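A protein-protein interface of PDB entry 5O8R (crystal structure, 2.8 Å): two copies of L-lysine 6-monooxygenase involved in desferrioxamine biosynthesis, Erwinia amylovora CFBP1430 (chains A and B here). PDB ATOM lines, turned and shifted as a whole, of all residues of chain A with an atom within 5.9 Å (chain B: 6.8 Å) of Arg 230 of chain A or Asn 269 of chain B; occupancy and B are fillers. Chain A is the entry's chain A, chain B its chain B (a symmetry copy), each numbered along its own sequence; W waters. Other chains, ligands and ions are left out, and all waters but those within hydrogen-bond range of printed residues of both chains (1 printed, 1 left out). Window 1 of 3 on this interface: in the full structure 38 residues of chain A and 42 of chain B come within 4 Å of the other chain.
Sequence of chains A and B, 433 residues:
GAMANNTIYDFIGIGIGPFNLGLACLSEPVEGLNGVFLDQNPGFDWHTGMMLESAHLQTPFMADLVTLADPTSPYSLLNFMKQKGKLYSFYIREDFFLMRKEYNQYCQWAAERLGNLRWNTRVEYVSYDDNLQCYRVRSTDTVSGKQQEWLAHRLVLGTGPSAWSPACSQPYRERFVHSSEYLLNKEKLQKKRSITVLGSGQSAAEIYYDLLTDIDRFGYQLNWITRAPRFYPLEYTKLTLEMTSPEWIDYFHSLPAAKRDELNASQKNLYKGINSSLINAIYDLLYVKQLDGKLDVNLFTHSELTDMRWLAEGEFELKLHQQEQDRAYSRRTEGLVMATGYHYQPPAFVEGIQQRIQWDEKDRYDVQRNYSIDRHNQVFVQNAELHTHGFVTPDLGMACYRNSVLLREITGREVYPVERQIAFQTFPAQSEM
The guanidinium group (NH1) of Arg 230 of chain A is in salt-bridge range of the side-chain carboxylate (OE1) of Glu 235 of chain B.
The side-chain hydroxyl (OG1) of Thr 240 of chain B sits at hydrogen-bond distance from the side-chain carboxylate (OE2) of Glu 235 of chain B. O of Asn 269 of chain B lies within hydrogen-bond range of N of Glu 235 of chain B, 2.9 Å away.
Arg 230 of chain A touches Met 243 of chain B. Asn 269 of chain B touches Arg 230 of chain A. Leu 270 of chain B touches Arg 230 of chain A (CD2 to CD, 3.9 Å). Gln 425 of chain B touches Phe 231 of chain A (OE1 to CE2, 3.8 Å). Tyr 232 of chain A touches Glu 235 of chain B (CB to OE2, 3.9 Å). Pro 233 of chain A touches Glu 235 of chain B (CD to CD, 3.4 Å).
Arg 230 of chain A touches four residues of chain B. Of the printed residues of chain A, Asn 269 of chain B touches Arg 230 (3.7 Å). Printed residues of chain B within 4 Å of Tyr 232 of chain A: Glu 235 (3.9 Å). Of the printed residues of chain A, Glu 235 of chain B touches Arg 230 (2.6 Å), Tyr 232 (3.9 Å) and Pro 233 (3.4 Å). Of the printed residues of chain A, Met 243 of chain B touches Arg 230. Of the printed residues of chain B, Pro 233 of chain A touches Glu 235 (3.4 Å). Thr 301 of chain A touches none of the printed residues of chain B. Pro 233 of chain B touches none of the printed residues of chain A. The nearest residue of chain B that does not touch Arg 230 of chain A is Thr 240 of chain B (4.3 Å). The nearest residue of chain A that does not touch Asn 269 of chain B is Asn 269 of chain A (5.5 Å). The nearest printed residue of chain B that does not touch Phe 231 of chain A is Thr 240 of chain B (4.4 Å).
Along chain B the printed residues that touch a printed residue of chain A span positions 235 to 425. Printed residues of chain A that touch a printed residue of chain B: Arg 230, Phe 231, Tyr 232 and Pro 233. Hydrophobic or aromatic side chains of chain A that line the printed part of chain B: Phe 231, Tyr 232 and Pro 233. Along chain A the printed residues that touch a printed residue of chain B span positions 230 to 233.
Arg 230 of chain A touches Asn 269 of chain B, but with the chains exchanged Asn 269 of chain A does not touch Arg 230 of chain B (4.3 Å). 4 positions are printed for both chains.
Water W1 bridges OG1 of Thr 240 of chain B (2.7 Å) and O of Phe 231 of chain A (2.8 Å).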
ATOM      1  N   SER A 200       2.801  -7.454  31.232  1.00  0.00           N
ATOM      2  CA  SER A 200       3.419  -6.211  30.729  1.00  0.00           C
ATOM      3  C   SER A 200       2.441  -5.194  30.176  1.00  0.00           C
ATOM      4  O   SER A 200       2.803  -4.347  29.348  1.00  0.00           O
ATOM      5  CB  SER A 200       4.529  -6.503  29.708  1.00  0.00           C
ATOM      6  OG  SER A 200       4.025  -7.161  28.560  1.00  0.00           O
ATOM      7  N   THR A 226       7.141 -11.176  31.196  1.00  0.00           N
ATOM      8  CA  THR A 226       5.869 -11.179  30.479  1.00  0.00           C
ATOM      9  C   THR A 226       5.819 -12.113  29.256  1.00  0.00           C
ATOM     10  O   THR A 226       6.829 -12.473  28.694  1.00  0.00           O
ATOM     11  CB  THR A 226       5.525  -9.775  30.035  1.00  0.00           C
ATOM     12  OG1 THR A 226       4.379  -9.812  29.190  1.00  0.00           O
ATOM     13  CG2 THR A 226       6.686  -9.178  29.280  1.00  0.00           C
ATOM     14  N   ALA A 228       4.292 -11.255  26.512  1.00  0.00           N
ATOM     15  CA  ALA A 228       4.305 -10.358  25.379  1.00  0.00           C
ATOM     16  C   ALA A 228       5.680 -10.339  24.804  1.00  0.00           C
ATOM     17  O   ALA A 228       6.641 -10.615  25.509  1.00  0.00           O
ATOM     18  CB  ALA A 228       3.940  -8.944  25.802  1.00  0.00           C
ATOM     19  N   PRO A 229       5.785 -10.009  23.518  1.00  0.00           N
ATOM     20  CA  PRO A 229       7.076  -9.977  22.821  1.00  0.00           C
ATOM     21  C   PRO A 229       8.013  -8.835  23.215  1.00  0.00           C
ATOM     22  O   PRO A 229       9.247  -8.999  23.215  1.00  0.00           O
ATOM     23  CB  PRO A 229       6.675  -9.865  21.354  1.00  0.00           C
ATOM     24  CG  PRO A 229       5.257  -9.366  21.366  1.00  0.00           C
ATOM     25  CD  PRO A 229       4.647  -9.948  22.583  1.00  0.00           C
ATOM     26  N   ARG A 230       7.430  -7.704  23.560  1.00  0.00           N
ATOM     27  CA  ARG A 230       8.176  -6.503  23.804  1.00  0.00           C
ATOM     28  C   ARG A 230       7.428  -5.817  24.906  1.00  0.00           C
ATOM     29  O   ARG A 230       6.241  -6.091  25.132  1.00  0.00           O
ATOM     30  CB  ARG A 230       8.207  -5.614  22.521  1.00  0.00           C
ATOM     31  CG  ARG A 230       9.110  -6.126  21.391  1.00  0.00           C
ATOM     32  CD  ARG A 230       8.816  -5.668  19.951  1.00  0.00           C
ATOM     33  NE  ARG A 230       7.462  -6.037  19.543  1.00  0.00           N
ATOM     34  CZ  ARG A 230       6.465  -5.177  19.313  1.00  0.00           C
ATOM     35  NH1 ARG A 230       6.661  -3.866  19.355  1.00  0.00           N
ATOM     36  NH2 ARG A 230       5.249  -5.631  19.005  1.00  0.00           N
ATOM     37  N   PHE A 231       8.091  -4.892  25.572  1.00  0.00           N
ATOM     38  CA  PHE A 231       7.384  -3.998  26.479  1.00  0.00           C
ATOM     39  C   PHE A 231       6.788  -2.891  25.629  1.00  0.00           C
ATOM     40  O   PHE A 231       7.203  -1.719  25.707  1.00  0.00           O
ATOM     41  CB  PHE A 231       8.336  -3.459  27.552  1.00  0.00           C
ATOM     42  CG  PHE A 231       8.859  -4.528  28.423  1.00  0.00           C
ATOM     43  CD1 PHE A 231       8.128  -4.990  29.475  1.00  0.00           C
ATOM     44  CD2 PHE A 231      10.032  -5.154  28.127  1.00  0.00           C
ATOM     45  CE1 PHE A 231       8.601  -5.983  30.281  1.00  0.00           C
ATOM     46  CE2 PHE A 231      10.492  -6.187  28.912  1.00  0.00           C
ATOM     47  CZ  PHE A 231       9.787  -6.571  30.008  1.00  0.00           C
ATOM     48  N   TYR A 232       5.825  -3.261  24.792  1.00  0.00           N
ATOM     49  CA  TYR A 232       5.389  -2.321  23.782  1.00  0.00           C
ATOM     50  C   TYR A 232       4.539  -1.139  24.311  1.00  0.00           C
ATOM     51  O   TYR A 232       3.697  -1.294  25.222  1.00  0.00           O
ATOM     52  CB  TYR A 232       4.716  -2.992  22.583  1.00  0.00           C
ATOM     53  CG  TYR A 232       3.640  -3.968  22.903  1.00  0.00           C
ATOM     54  CD1 TYR A 232       2.450  -3.549  23.447  1.00  0.00           C
ATOM     55  CD2 TYR A 232       3.798  -5.302  22.612  1.00  0.00           C
ATOM     56  CE1 TYR A 232       1.452  -4.457  23.744  1.00  0.00           C
ATOM     57  CE2 TYR A 232       2.816  -6.217  22.881  1.00  0.00           C
ATOM     58  CZ  TYR A 232       1.636  -5.810  23.461  1.00  0.00           C
ATOM     59  OH  TYR A 232       0.649  -6.750  23.766  1.00  0.00           O
ATOM     60  N   PRO A 233       4.746   0.032  23.701  1.00  0.00           N
ATOM     61  CA  PRO A 233       3.897   1.160  23.976  1.00  0.00           C
ATOM     62  C   PRO A 233       2.515   1.006  23.362  1.00  0.00           C
ATOM     63  O   PRO A 233       2.352   0.370  22.317  1.00  0.00           O
ATOM     64  CB  PRO A 233       4.630   2.324  23.290  1.00  0.00           C
ATOM     65  CG  PRO A 233       5.268   1.675  22.119  1.00  0.00           C
ATOM     66  CD  PRO A 233       5.661   0.305  22.577  1.00  0.00           C
ATOM     67  N   ASN A 269      -1.508  -4.022  20.651  1.00  0.00           N
ATOM     68  CA  ASN A 269      -0.841  -2.757  21.078  1.00  0.00           C
ATOM     69  C   ASN A 269      -1.653  -1.461  20.850  1.00  0.00           C
ATOM     70  O   ASN A 269      -1.122  -0.351  21.057  1.00  0.00           O
ATOM     71  CB  ASN A 269       0.614  -2.646  20.509  1.00  0.00           C
ATOM     72  CG  ASN A 269       0.692  -2.126  19.069  1.00  0.00           C
ATOM     73  OD1 ASN A 269       0.326  -2.816  18.124  1.00  0.00           O
ATOM     74  ND2 ASN A 269       1.239  -0.920  18.904  1.00  0.00           N
ATOM     75  N   THR A 301      10.926 -11.570  28.562  1.00  0.00           N
ATOM     76  CA  THR A 301       9.962 -11.215  27.552  1.00  0.00           C
ATOM     77  C   THR A 301       9.639 -12.512  26.700  1.00  0.00           C
ATOM     78  O   THR A 301      10.288 -13.549  26.860  1.00  0.00           O
ATOM     79  CB  THR A 301      10.581 -10.002  26.828  1.00  0.00           C
ATOM     80  OG1 THR A 301       9.620  -9.398  25.992  1.00  0.00           O
ATOM     81  CG2 THR A 301      11.872 -10.384  26.024  1.00  0.00           C
ATOM     82  N   HIS A 302       8.605 -12.503  25.867  1.00  0.00           N
ATOM     83  CA  HIS A 302       8.134 -13.746  25.172  1.00  0.00           C
ATOM     84  C   HIS A 302       7.856 -14.972  26.051  1.00  0.00           C
ATOM     85  O   HIS A 302       7.920 -16.082  25.542  1.00  0.00           O
ATOM     86  CB  HIS A 302       9.103 -14.216  24.067  1.00  0.00           C
ATOM     87  CG  HIS A 302       9.275 -13.258  22.939  1.00  0.00           C
ATOM     88  ND1 HIS A 302      10.375 -12.427  22.834  1.00  0.00           N
ATOM     89  CD2 HIS A 302       8.494 -13.005  21.857  1.00  0.00           C
ATOM     90  CE1 HIS A 302      10.281 -11.725  21.718  1.00  0.00           C
ATOM     91  NE2 HIS A 302       9.143 -12.041  21.119  1.00  0.00           N
ATOM     92  N   ARG B 230      -1.833  -0.209   8.803  1.00  0.00           N
ATOM     93  CA  ARG B 230      -1.922   1.086   9.407  1.00  0.00           C
ATOM     94  C   ARG B 230      -0.747   1.960   9.013  1.00  0.00           C
ATOM     95  O   ARG B 230       0.325   1.478   8.599  1.00  0.00           O
ATOM     96  CB  ARG B 230      -1.793   0.913  10.879  1.00  0.00           C
ATOM     97  CG  ARG B 230      -2.832   0.071  11.536  1.00  0.00           C
ATOM     98  CD  ARG B 230      -2.673   0.219  13.051  1.00  0.00           C
ATOM     99  NE  ARG B 230      -1.364  -0.258  13.491  1.00  0.00           N
ATOM    100  CZ  ARG B 230      -1.014  -1.545  13.552  1.00  0.00           C
ATOM    101  NH1 ARG B 230      -1.884  -2.523  13.217  1.00  0.00           N
ATOM    102  NH2 ARG B 230       0.225  -1.858  13.930  1.00  0.00           N
ATOM    103  N   TYR B 232       1.808   3.082  10.554  1.00  0.00           N
ATOM    104  CA  TYR B 232       2.374   2.797  11.871  1.00  0.00           C
ATOM    105  C   TYR B 232       3.652   3.518  12.149  1.00  0.00           C
ATOM    106  O   TYR B 232       4.444   3.799  11.241  1.00  0.00           O
ATOM    107  CB  TYR B 232       2.558   1.311  12.198  1.00  0.00           C
ATOM    108  CG  TYR B 232       3.272   0.463  11.197  1.00  0.00           C
ATOM    109  CD1 TYR B 232       4.598   0.684  10.857  1.00  0.00           C
ATOM    110  CD2 TYR B 232       2.627  -0.624  10.640  1.00  0.00           C
ATOM    111  CE1 TYR B 232       5.243  -0.129   9.930  1.00  0.00           C
ATOM    112  CE2 TYR B 232       3.251  -1.439   9.726  1.00  0.00           C
ATOM    113  CZ  TYR B 232       4.553  -1.196   9.365  1.00  0.00           C
ATOM    114  OH  TYR B 232       5.117  -2.042   8.440  1.00  0.00           O
ATOM    115  N   PRO B 233       3.867   3.793  13.422  1.00  0.00           N
ATOM    116  CA  PRO B 233       5.106   4.385  13.838  1.00  0.00           C
ATOM    117  C   PRO B 233       6.219   3.348  14.045  1.00  0.00           C
ATOM    118  O   PRO B 233       5.977   2.226  14.477  1.00  0.00           O
ATOM    119  CB  PRO B 233       4.737   5.048  15.161  1.00  0.00           C
ATOM    120  CG  PRO B 233       3.686   4.125  15.729  1.00  0.00           C
ATOM    121  CD  PRO B 233       2.916   3.644  14.543  1.00  0.00           C
ATOM    122  N   LEU B 234       7.432   3.766  13.720  1.00  0.00           N
ATOM    123  CA  LEU B 234       8.635   3.124  14.161  1.00  0.00           C
ATOM    124  C   LEU B 234       8.617   3.181  15.694  1.00  0.00           C
ATOM    125  O   LEU B 234       8.610   4.265  16.278  1.00  0.00           O
ATOM    126  CB  LEU B 234       9.837   3.894  13.630  1.00  0.00           C
ATOM    127  CG  LEU B 234      11.161   3.168  13.765  1.00  0.00           C
ATOM    128  CD1 LEU B 234      11.271   2.218  12.578  1.00  0.00           C
ATOM    129  CD2 LEU B 234      12.376   4.116  13.885  1.00  0.00           C
ATOM    130  N   GLU B 235       8.589   2.012  16.324  1.00  0.00           N
ATOM    131  CA  GLU B 235       8.601   1.907  17.758  1.00  0.00           C
ATOM    132  C   GLU B 235       9.934   2.341  18.347  1.00  0.00           C
ATOM    133  O   GLU B 235      10.896   1.648  18.187  1.00  0.00           O
ATOM    134  CB  GLU B 235       8.323   0.464  18.149  1.00  0.00           C
ATOM    135  CG  GLU B 235       7.986   0.296  19.633  1.00  0.00           C
ATOM    136  CD  GLU B 235       7.354  -1.054  19.924  1.00  0.00           C
ATOM    137  OE1 GLU B 235       6.250  -1.288  19.363  1.00  0.00           O
ATOM    138  OE2 GLU B 235       7.972  -1.888  20.670  1.00  0.00           O
ATOM    139  N   TYR B 236       9.960   3.459  19.071  1.00  0.00           N
ATOM    140  CA  TYR B 236      11.200   4.110  19.515  1.00  0.00           C
ATOM    141  C   TYR B 236      11.297   4.311  21.072  1.00  0.00           C
ATOM    142  O   TYR B 236      12.193   5.066  21.623  1.00  0.00           O
ATOM    143  CB  TYR B 236      11.317   5.424  18.761  1.00  0.00           C
ATOM    144  CG  TYR B 236      12.701   6.029  18.689  1.00  0.00           C
ATOM    145  CD1 TYR B 236      13.683   5.475  17.865  1.00  0.00           C
ATOM    146  CD2 TYR B 236      13.024   7.228  19.415  1.00  0.00           C
ATOM    147  CE1 TYR B 236      14.960   6.054  17.809  1.00  0.00           C
ATOM    148  CE2 TYR B 236      14.281   7.822  19.355  1.00  0.00           C
ATOM    149  CZ  TYR B 236      15.247   7.225  18.564  1.00  0.00           C
ATOM    150  OH  TYR B 236      16.516   7.739  18.485  1.00  0.00           O
ATOM    151  N   THR B 240      12.173  -0.965  24.019  1.00  0.00           N
ATOM    152  CA  THR B 240      12.342  -1.567  22.671  1.00  0.00           C
ATOM    153  C   THR B 240      13.648  -1.221  21.967  1.00  0.00           C
ATOM    154  O   THR B 240      14.151  -2.063  21.263  1.00  0.00           O
ATOM    155  CB  THR B 240      11.198  -1.236  21.721  1.00  0.00           C
ATOM    156  OG1 THR B 240       9.970  -1.662  22.316  1.00  0.00           O
ATOM    157  CG2 THR B 240      11.355  -1.982  20.442  1.00  0.00           C
ATOM    158  N   MET B 243      16.532  -3.713  21.970  1.00  0.00           N
ATOM    159  CA  MET B 243      16.557  -4.814  21.024  1.00  0.00           C
ATOM    160  C   MET B 243      17.651  -4.573  19.995  1.00  0.00           C
ATOM    161  O   MET B 243      18.079  -5.488  19.357  1.00  0.00           O
ATOM    162  CB  MET B 243      15.203  -4.983  20.334  1.00  0.00           C
ATOM    163  CG  MET B 243      14.143  -5.548  21.241  1.00  0.00           C
ATOM    164  SD  MET B 243      12.508  -5.790  20.495  1.00  0.00           S
ATOM    165  CE  MET B 243      12.848  -7.080  19.309  1.00  0.00           C
ATOM    166  N   ASN B 264      11.186 -11.234  10.694  1.00  0.00           N
ATOM    167  CA  ASN B 264      11.520 -10.030   9.939  1.00  0.00           C
ATOM    168  C   ASN B 264      10.309  -9.420   9.205  1.00  0.00           C
ATOM    169  O   ASN B 264      10.210  -8.188   9.088  1.00  0.00           O
ATOM    170  CB  ASN B 264      12.699 -10.281   8.988  1.00  0.00           C
ATOM    171  CG  ASN B 264      14.043 -10.177   9.677  1.00  0.00           C
ATOM    172  OD1 ASN B 264      14.226  -9.490  10.722  1.00  0.00           O
ATOM    173  ND2 ASN B 264      15.007 -10.873   9.106  1.00  0.00           N
ATOM    174  N   ALA B 265       9.384 -10.265   8.739  1.00  0.00           N
ATOM    175  CA  ALA B 265       8.130  -9.757   8.183  1.00  0.00           C
ATOM    176  C   ALA B 265       7.132  -9.334   9.295  1.00  0.00           C
ATOM    177  O   ALA B 265       6.344  -8.408   9.073  1.00  0.00           O
ATOM    178  CB  ALA B 265       7.511 -10.759   7.216  1.00  0.00           C
ATOM    179  N   SER B 266       7.172  -9.979  10.473  1.00  0.00           N
ATOM    180  CA  SER B 266       6.306  -9.579  11.623  1.00  0.00           C
ATOM    181  C   SER B 266       6.771  -8.325  12.409  1.00  0.00           C
ATOM    182  O   SER B 266       5.938  -7.614  12.958  1.00  0.00           O
ATOM    183  CB  SER B 266       6.028 -10.766  12.582  1.00  0.00           C
ATOM    184  OG  SER B 266       7.112 -11.063  13.449  1.00  0.00           O
ATOM    185  N   GLN B 267       8.076  -8.056  12.435  1.00  0.00           N
ATOM    186  CA  GLN B 267       8.667  -6.891  13.113  1.00  0.00           C
ATOM    187  C   GLN B 267       8.911  -5.657  12.207  1.00  0.00           C
ATOM    188  O   GLN B 267       9.885  -4.907  12.449  1.00  0.00           O
ATOM    189  CB  GLN B 267      10.042  -7.258  13.686  1.00  0.00           C
ATOM    190  CG  GLN B 267      10.143  -8.451  14.618  1.00  0.00           C
ATOM    191  CD  GLN B 267      11.589  -8.711  15.052  1.00  0.00           C
ATOM    192  OE1 GLN B 267      12.582  -8.501  14.295  1.00  0.00           O
ATOM    193  NE2 GLN B 267      11.719  -9.159  16.282  1.00  0.00           N
ATOM    194  N   LYS B 268       8.082  -5.415  11.187  1.00  0.00           N
ATOM    195  CA  LYS B 268       8.387  -4.280  10.298  1.00  0.00           C
ATOM    196  C   LYS B 268       8.339  -2.890  11.026  1.00  0.00           C
ATOM    197  O   LYS B 268       9.066  -1.938  10.642  1.00  0.00           O
ATOM    198  CB  LYS B 268       7.525  -4.311   9.024  1.00  0.00           C
ATOM    199  CG  LYS B 268       8.101  -5.175   7.887  1.00  0.00           C
ATOM    200  CD  LYS B 268       7.172  -5.295   6.670  1.00  0.00           C
ATOM    201  CE  LYS B 268       5.820  -5.925   7.031  1.00  0.00           C
ATOM    202  NZ  LYS B 268       5.449  -7.111   6.203  1.00  0.00           N
ATOM    203  N   ASN B 269       7.536  -2.802  12.097  1.00  0.00           N
ATOM    204  CA  ASN B 269       7.445  -1.590  12.938  1.00  0.00           C
ATOM    205  C   ASN B 269       8.678  -1.259  13.800  1.00  0.00           C
ATOM    206  O   ASN B 269       8.692  -0.207  14.441  1.00  0.00           O
ATOM    207  CB  ASN B 269       6.225  -1.662  13.851  1.00  0.00           C
ATOM    208  CG  ASN B 269       6.437  -2.579  15.041  1.00  0.00           C
ATOM    209  OD1 ASN B 269       7.103  -3.616  14.940  1.00  0.00           O
ATOM    210  ND2 ASN B 269       5.877  -2.197  16.180  1.00  0.00           N
ATOM    211  N   LEU B 270       9.672  -2.155  13.839  1.00  0.00           N
ATOM    212  CA  LEU B 270      10.953  -1.868  14.489  1.00  0.00           C
ATOM    213  C   LEU B 270      11.969  -1.119  13.632  1.00  0.00           C
ATOM    214  O   LEU B 270      12.860  -0.438  14.159  1.00  0.00           O
ATOM    215  CB  LEU B 270      11.613  -3.157  14.980  1.00  0.00           C
ATOM    216  CG  LEU B 270      10.883  -4.087  15.963  1.00  0.00           C
ATOM    217  CD1 LEU B 270      11.886  -4.989  16.652  1.00  0.00           C
ATOM    218  CD2 LEU B 270      10.084  -3.358  17.030  1.00  0.00           C
ATOM    219  N   TYR B 271      11.868  -1.270  12.320  1.00  0.00           N
ATOM    220  CA  TYR B 271      12.828  -0.629  11.398  1.00  0.00           C
ATOM    221  C   TYR B 271      12.228   0.053  10.167  1.00  0.00           C
ATOM    222  O   TYR B 271      12.888   0.884   9.582  1.00  0.00           O
ATOM    223  CB  TYR B 271      13.903  -1.622  10.965  1.00  0.00           C
ATOM    224  CG  TYR B 271      13.446  -2.815  10.093  1.00  0.00           C
ATOM    225  CD1 TYR B 271      12.518  -3.771  10.555  1.00  0.00           C
ATOM    226  CD2 TYR B 271      13.998  -3.022   8.824  1.00  0.00           C
ATOM    227  CE1 TYR B 271      12.145  -4.867   9.777  1.00  0.00           C
ATOM    228  CE2 TYR B 271      13.634  -4.116   8.052  1.00  0.00           C
ATOM    229  CZ  TYR B 271      12.713  -5.033   8.533  1.00  0.00           C
ATOM    230  OH  TYR B 271      12.378  -6.098   7.746  1.00  0.00           O
ATOM    231  N   LYS B 272      10.991  -0.276   9.784  1.00  0.00           N
ATOM    232  CA  LYS B 272      10.409   0.256   8.561  1.00  0.00           C
ATOM    233  C   LYS B 272       9.395   1.374   8.760  1.00  0.00           C
ATOM    234  O   LYS B 272       9.165   2.112   7.817  1.00  0.00           O
ATOM    235  CB  LYS B 272       9.820  -0.877   7.701  1.00  0.00           C
ATOM    236  CG  LYS B 272      10.885  -1.638   6.891  1.00  0.00           C
ATOM    237  CD  LYS B 272      10.278  -2.519   5.790  1.00  0.00           C
ATOM    238  CE  LYS B 272      11.237  -2.692   4.621  1.00  0.00           C
ATOM    239  NZ  LYS B 272      12.488  -3.421   4.964  1.00  0.00           N
ATOM    240  N   GLY B 273       8.832   1.536   9.956  1.00  0.00           N
ATOM    241  CA  GLY B 273       7.779   2.531  10.183  1.00  0.00           C
ATOM    242  C   GLY B 273       8.162   4.025  10.177  1.00  0.00           C
ATOM    243  O   GLY B 273       9.329   4.414  10.061  1.00  0.00           O
ATOM    244  N   ILE B 274       7.147   4.863  10.340  1.00  0.00           N
ATOM    245  CA  ILE B 274       7.268   6.300  10.226  1.00  0.00           C
ATOM    246  C   ILE B 274       7.594   6.883  11.572  1.00  0.00           C
ATOM    247  O   ILE B 274       6.997   6.507  12.553  1.00  0.00           O
ATOM    248  CB  ILE B 274       5.923   6.887   9.806  1.00  0.00           C
ATOM    249  CG1 ILE B 274       5.414   6.135   8.563  1.00  0.00           C
ATOM    250  CG2 ILE B 274       6.064   8.363   9.468  1.00  0.00           C
ATOM    251  CD1 ILE B 274       4.008   6.465   8.122  1.00  0.00           C
ATOM    252  N   GLN B 425      17.639  -5.816  29.905  1.00  0.00           N
ATOM    253  CA  GLN B 425      16.921  -7.045  29.821  1.00  0.00           C
ATOM    254  C   GLN B 425      17.728  -8.180  29.270  1.00  0.00           C
ATOM    255  O   GLN B 425      18.837  -8.026  28.840  1.00  0.00           O
ATOM    256  CB  GLN B 425      15.649  -6.939  29.038  1.00  0.00           C
ATOM    257  CG  GLN B 425      15.555  -5.782  28.090  1.00  0.00           C
ATOM    258  CD  GLN B 425      14.390  -5.949  27.165  1.00  0.00           C
ATOM    259  OE1 GLN B 425      13.776  -6.981  27.120  1.00  0.00           O
ATOM    260  NE2 GLN B 425      14.079  -4.911  26.422  1.00  0.00           N
HETATM  261  O   HOH W   1       9.233  -0.258  24.528  1.00  0.00           O
